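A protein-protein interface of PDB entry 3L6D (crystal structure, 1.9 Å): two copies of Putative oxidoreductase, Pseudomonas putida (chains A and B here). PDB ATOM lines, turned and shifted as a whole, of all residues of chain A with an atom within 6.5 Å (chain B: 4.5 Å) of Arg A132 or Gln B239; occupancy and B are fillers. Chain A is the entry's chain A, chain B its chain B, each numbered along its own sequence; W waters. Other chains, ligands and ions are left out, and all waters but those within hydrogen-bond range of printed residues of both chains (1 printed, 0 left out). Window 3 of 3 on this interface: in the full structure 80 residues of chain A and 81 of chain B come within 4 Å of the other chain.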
ATOM      1  N   ILE A  23      20.164  -8.262   6.818  1.00  0.00           N
ATOM      2  CA  ILE A  23      19.008  -7.998   5.950  1.00  0.00           C
ATOM      3  C   ILE A  23      19.209  -8.612   4.586  1.00  0.00           C
ATOM      4  O   ILE A  23      18.271  -9.165   4.031  1.00  0.00           O
ATOM      5  CB  ILE A  23      18.736  -6.466   5.672  1.00  0.00           C
ATOM      6  CG1 ILE A  23      19.140  -5.567   6.845  1.00  0.00           C
ATOM      7  CG2 ILE A  23      17.257  -6.274   5.232  1.00  0.00           C
ATOM      8  CD1 ILE A  23      18.193  -5.578   8.017  1.00  0.00           C
ATOM      9  N   ALA A 129      20.297   2.196  -0.977  1.00  0.00           N
ATOM     10  CA  ALA A 129      19.112   1.980  -0.210  1.00  0.00           C
ATOM     11  C   ALA A 129      19.437   1.948   1.249  1.00  0.00           C
ATOM     12  O   ALA A 129      20.500   1.565   1.630  1.00  0.00           O
ATOM     13  CB  ALA A 129      18.520   0.701  -0.585  1.00  0.00           C
ATOM     14  N   TYR A 130      18.465   2.321   2.044  1.00  0.00           N
ATOM     15  CA  TYR A 130      18.457   1.999   3.473  1.00  0.00           C
ATOM     16  C   TYR A 130      18.084   0.518   3.635  1.00  0.00           C
ATOM     17  O   TYR A 130      17.503  -0.071   2.727  1.00  0.00           O
ATOM     18  CB  TYR A 130      17.517   2.969   4.214  1.00  0.00           C
ATOM     19  CG  TYR A 130      18.073   4.380   4.246  1.00  0.00           C
ATOM     20  CD1 TYR A 130      19.123   4.707   5.098  1.00  0.00           C
ATOM     21  CD2 TYR A 130      17.578   5.376   3.415  1.00  0.00           C
ATOM     22  CE1 TYR A 130      19.657   6.018   5.121  1.00  0.00           C
ATOM     23  CE2 TYR A 130      18.103   6.687   3.436  1.00  0.00           C
ATOM     24  CZ  TYR A 130      19.144   6.982   4.289  1.00  0.00           C
ATOM     25  OH  TYR A 130      19.683   8.250   4.353  1.00  0.00           O
ATOM     26  N   PRO A 131      18.483  -0.118   4.757  1.00  0.00           N
ATOM     27  CA  PRO A 131      18.235  -1.556   4.926  1.00  0.00           C
ATOM     28  C   PRO A 131      16.790  -1.959   4.719  1.00  0.00           C
ATOM     29  O   PRO A 131      16.529  -3.012   4.113  1.00  0.00           O
ATOM     30  CB  PRO A 131      18.676  -1.801   6.379  1.00  0.00           C
ATOM     31  CG  PRO A 131      19.883  -0.915   6.505  1.00  0.00           C
ATOM     32  CD  PRO A 131      19.474   0.368   5.753  1.00  0.00           C
ATOM     33  N   ARG A 132      15.862  -1.116   5.169  1.00  0.00           N
ATOM     34  CA  ARG A 132      14.439  -1.396   4.987  1.00  0.00           C
ATOM     35  C   ARG A 132      14.080  -1.586   3.515  1.00  0.00           C
ATOM     36  O   ARG A 132      13.112  -2.266   3.236  1.00  0.00           O
ATOM     37  CB  ARG A 132      13.545  -0.322   5.650  1.00  0.00           C
ATOM     38  CG  ARG A 132      13.735   1.081   5.110  1.00  0.00           C
ATOM     39  CD  ARG A 132      12.613   2.022   5.517  1.00  0.00           C
ATOM     40  NE  ARG A 132      12.715   3.284   4.789  1.00  0.00           N
ATOM     41  CZ  ARG A 132      13.604   4.229   5.065  1.00  0.00           C
ATOM     42  NH1 ARG A 132      14.462   4.055   6.056  1.00  0.00           N
ATOM     43  NH2 ARG A 132      13.615   5.353   4.366  1.00  0.00           N
ATOM     44  N   ASN A 133      14.855  -1.027   2.566  1.00  0.00           N
ATOM     45  CA  ASN A 133      14.539  -1.262   1.146  1.00  0.00           C
ATOM     46  C   ASN A 133      15.476  -2.212   0.381  1.00  0.00           C
ATOM     47  O   ASN A 133      15.374  -2.369  -0.852  1.00  0.00           O
ATOM     48  CB  ASN A 133      14.396   0.070   0.389  1.00  0.00           C
ATOM     49  CG  ASN A 133      13.226   0.860   0.882  1.00  0.00           C
ATOM     50  OD1 ASN A 133      12.139   0.302   1.025  1.00  0.00           O
ATOM     51  ND2 ASN A 133      13.438   2.154   1.195  1.00  0.00           N
ATOM     52  N   VAL A 134      16.375  -2.873   1.093  1.00  0.00           N
ATOM     53  CA  VAL A 134      17.043  -4.023   0.470  1.00  0.00           C
ATOM     54  C   VAL A 134      15.978  -5.026   0.007  1.00  0.00           C
ATOM     55  O   VAL A 134      15.042  -5.331   0.755  1.00  0.00           O
ATOM     56  CB  VAL A 134      18.053  -4.707   1.418  1.00  0.00           C
ATOM     57  CG1 VAL A 134      18.635  -5.976   0.769  1.00  0.00           C
ATOM     58  CG2 VAL A 134      19.151  -3.736   1.822  1.00  0.00           C
ATOM     59  N   GLY A 135      16.091  -5.495  -1.232  1.00  0.00           N
ATOM     60  CA  GLY A 135      15.080  -6.395  -1.833  1.00  0.00           C
ATOM     61  C   GLY A 135      13.982  -5.718  -2.644  1.00  0.00           C
ATOM     62  O   GLY A 135      13.228  -6.370  -3.398  1.00  0.00           O
ATOM     63  N   HIS A 136      13.875  -4.403  -2.480  1.00  0.00           N
ATOM     64  CA  HIS A 136      12.789  -3.687  -3.092  1.00  0.00           C
ATOM     65  C   HIS A 136      13.023  -3.646  -4.577  1.00  0.00           C
ATOM     66  O   HIS A 136      14.144  -3.367  -5.011  1.00  0.00           O
ATOM     67  CB  HIS A 136      12.713  -2.272  -2.530  1.00  0.00           C
ATOM     68  CG  HIS A 136      11.392  -1.619  -2.738  1.00  0.00           C
ATOM     69  ND1 HIS A 136      10.919  -1.283  -3.983  1.00  0.00           N
ATOM     70  CD2 HIS A 136      10.443  -1.233  -1.851  1.00  0.00           C
ATOM     71  CE1 HIS A 136       9.726  -0.716  -3.857  1.00  0.00           C
ATOM     72  NE2 HIS A 136       9.426  -0.657  -2.570  1.00  0.00           N
ATOM     73  N   ASP B 221      11.513   7.999  -1.108  1.00  0.00           N
ATOM     74  CA  ASP B 221      11.237   7.124   0.031  1.00  0.00           C
ATOM     75  C   ASP B 221      11.847   7.733   1.299  1.00  0.00           C
ATOM     76  O   ASP B 221      11.224   7.676   2.371  1.00  0.00           O
ATOM     77  CB  ASP B 221      11.791   5.722  -0.228  1.00  0.00           C
ATOM     78  CG  ASP B 221      11.765   4.833   1.022  1.00  0.00           C
ATOM     79  OD1 ASP B 221      12.709   4.874   1.832  1.00  0.00           O
ATOM     80  OD2 ASP B 221      10.809   4.079   1.156  1.00  0.00           O
ATOM     81  N   ALA B 222      13.028   8.344   1.176  1.00  0.00           N
ATOM     82  CA  ALA B 222      13.690   9.028   2.325  1.00  0.00           C
ATOM     83  C   ALA B 222      12.894  10.242   2.855  1.00  0.00           C
ATOM     84  O   ALA B 222      12.714  10.383   4.072  1.00  0.00           O
ATOM     85  CB  ALA B 222      15.115   9.434   1.985  1.00  0.00           C
ATOM     86  N   GLU B 225       9.712   8.952   4.587  1.00  0.00           N
ATOM     87  CA  GLU B 225      10.027   8.445   5.882  1.00  0.00           C
ATOM     88  C   GLU B 225      10.367   9.570   6.893  1.00  0.00           C
ATOM     89  O   GLU B 225       9.962   9.497   8.054  1.00  0.00           O
ATOM     90  CB  GLU B 225      11.122   7.383   5.780  1.00  0.00           C
ATOM     91  CG  GLU B 225      11.669   6.944   7.122  1.00  0.00           C
ATOM     92  CD  GLU B 225      10.742   6.032   7.949  1.00  0.00           C
ATOM     93  OE1 GLU B 225       9.635   5.642   7.488  1.00  0.00           O
ATOM     94  OE2 GLU B 225      11.172   5.708   9.092  1.00  0.00           O
ATOM     95  N   LYS B 236      14.347   7.920  16.766  1.00  0.00           N
ATOM     96  CA  LYS B 236      15.202   6.822  17.230  1.00  0.00           C
ATOM     97  C   LYS B 236      16.199   6.494  16.133  1.00  0.00           C
ATOM     98  O   LYS B 236      15.823   6.344  14.964  1.00  0.00           O
ATOM     99  CB  LYS B 236      14.388   5.580  17.607  1.00  0.00           C
ATOM    100  CG  LYS B 236      13.437   5.753  18.792  1.00  0.00           C
ATOM    101  CD  LYS B 236      12.330   4.670  18.769  1.00  0.00           C
ATOM    102  CE  LYS B 236      11.202   4.938  19.782  1.00  0.00           C
ATOM    103  NZ  LYS B 236      10.060   3.966  19.640  1.00  0.00           N
ATOM    104  N   GLY B 237      17.455   6.318  16.522  1.00  0.00           N
ATOM    105  CA  GLY B 237      18.537   6.112  15.593  1.00  0.00           C
ATOM    106  C   GLY B 237      18.643   4.682  15.149  1.00  0.00           C
ATOM    107  O   GLY B 237      19.695   4.184  14.815  1.00  0.00           O
ATOM    108  N   ASP B 238      17.510   4.016  15.104  1.00  0.00           N
ATOM    109  CA  ASP B 238      17.523   2.658  14.670  1.00  0.00           C
ATOM    110  C   ASP B 238      17.977   2.477  13.258  1.00  0.00           C
ATOM    111  O   ASP B 238      18.659   1.527  12.977  1.00  0.00           O
ATOM    112  CB  ASP B 238      16.191   1.941  14.921  1.00  0.00           C
ATOM    113  CG  ASP B 238      15.001   2.607  14.249  1.00  0.00           C
ATOM    114  OD1 ASP B 238      14.482   3.590  14.792  1.00  0.00           O
ATOM    115  OD2 ASP B 238      14.536   2.105  13.207  1.00  0.00           O
ATOM    116  N   GLN B 239      17.565   3.308  12.326  1.00  0.00           N
ATOM    117  CA  GLN B 239      17.973   3.049  10.942  1.00  0.00           C
ATOM    118  C   GLN B 239      19.038   3.911  10.198  1.00  0.00           C
ATOM    119  O   GLN B 239      19.822   3.411   9.414  1.00  0.00           O
ATOM    120  CB  GLN B 239      16.706   2.926  10.115  1.00  0.00           C
ATOM    121  CG  GLN B 239      16.917   2.673   8.662  1.00  0.00           C
ATOM    122  CD  GLN B 239      15.916   1.695   8.101  1.00  0.00           C
ATOM    123  OE1 GLN B 239      16.195   0.970   7.186  1.00  0.00           O
ATOM    124  NE2 GLN B 239      14.735   1.700   8.661  1.00  0.00           N
ATOM    125  N   ALA B 240      18.986   5.211  10.415  1.00  0.00           N
ATOM    126  CA  ALA B 240      19.786   6.180   9.731  1.00  0.00           C
ATOM    127  C   ALA B 240      20.397   7.186  10.673  1.00  0.00           C
ATOM    128  O   ALA B 240      19.914   8.274  10.743  1.00  0.00           O
ATOM    129  CB  ALA B 240      18.957   6.860   8.734  1.00  0.00           C
ATOM    130  N   ARG B 241      21.428   6.828  11.408  1.00  0.00           N
ATOM    131  CA  ARG B 241      22.001   7.741  12.370  1.00  0.00           C
ATOM    132  C   ARG B 241      22.553   8.998  11.763  1.00  0.00           C
ATOM    133  O   ARG B 241      23.199   8.977  10.773  1.00  0.00           O
ATOM    134  CB  ARG B 241      23.107   7.056  13.162  1.00  0.00           C
ATOM    135  CG  ARG B 241      22.608   6.046  14.124  1.00  0.00           C
ATOM    136  CD  ARG B 241      23.718   5.420  14.910  1.00  0.00           C
ATOM    137  NE  ARG B 241      24.544   6.397  15.575  1.00  0.00           N
ATOM    138  CZ  ARG B 241      24.718   6.436  16.877  1.00  0.00           C
ATOM    139  NH1 ARG B 241      24.098   5.561  17.640  1.00  0.00           N
ATOM    140  NH2 ARG B 241      25.495   7.350  17.410  1.00  0.00           N
HETATM  141  O   HOH W   1      10.453   2.852   3.495  1.00  0.00           O
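The backbone NH (N) of Arg A132 lies within hydrogen-bond range of the side-chain amide oxygen (OE1) of Gln B239 (2.9 Å).
The side-chain amide nitrogen of Asn A133 sits at hydrogen-bond distance from the side-chain carboxylate of Asp B221 (2.9 Å).
The guanidinium group (NH2) of Arg A132 is in salt-bridge range of the side-chain carboxylate (OD1) of Asp B221, 2.7 Å away.
CB of Tyr A130 touches OE1 of Gln B239, 3.8 Å away.
Tyr A130 touches Ala B240.
Pro A131 touches Gln B239 (N to OE1, 3.5 Å).
Arg A132 touches Glu B225.
Arg A132 touches three residues of chain B.
Printed residues of chain A within 4 Å of Gln B239: Tyr A130, Pro A131 and Arg A132.
Of the printed residues of chain B, Asn A133 touches Asp B221 (2.9 Å).
Of the printed residues of chain B, Tyr A130 touches Gln B239 (3.8 Å) and Ala B240 (3.8 Å).
Ala A129 touches none of the printed residues of chain B.
The nearest residue of chain B that does not touch Arg A132 is Ala B222 (4.2 Å).
The nearest residue of chain A that does not touch Gln B239 is Asn A133 (5.2 Å).
The nearest printed residue of chain A that does not touch Asp B221 is Tyr A130 (5.1 Å).
Of the 9 printed residues of chain B, 4 touch a printed residue of chain A.
Of the 9 printed residues of chain A, 4 touch a printed residue of chain B.
Among the printed residues, 7 pairs touch across the chains.
Among the printed residues, Asp or Glu carboxylates within 4 Å of a Lys or Arg side-chain nitrogen of the other chain: Arg A132 with Asp B221 (2.7 Å).
No position is printed for both chains.
Water W1 bridges the guanidinium group (NE) of Arg A132 (2.6 Å) and the side-chain carboxylate (OD2) of Asp B221 (2.7 Å).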
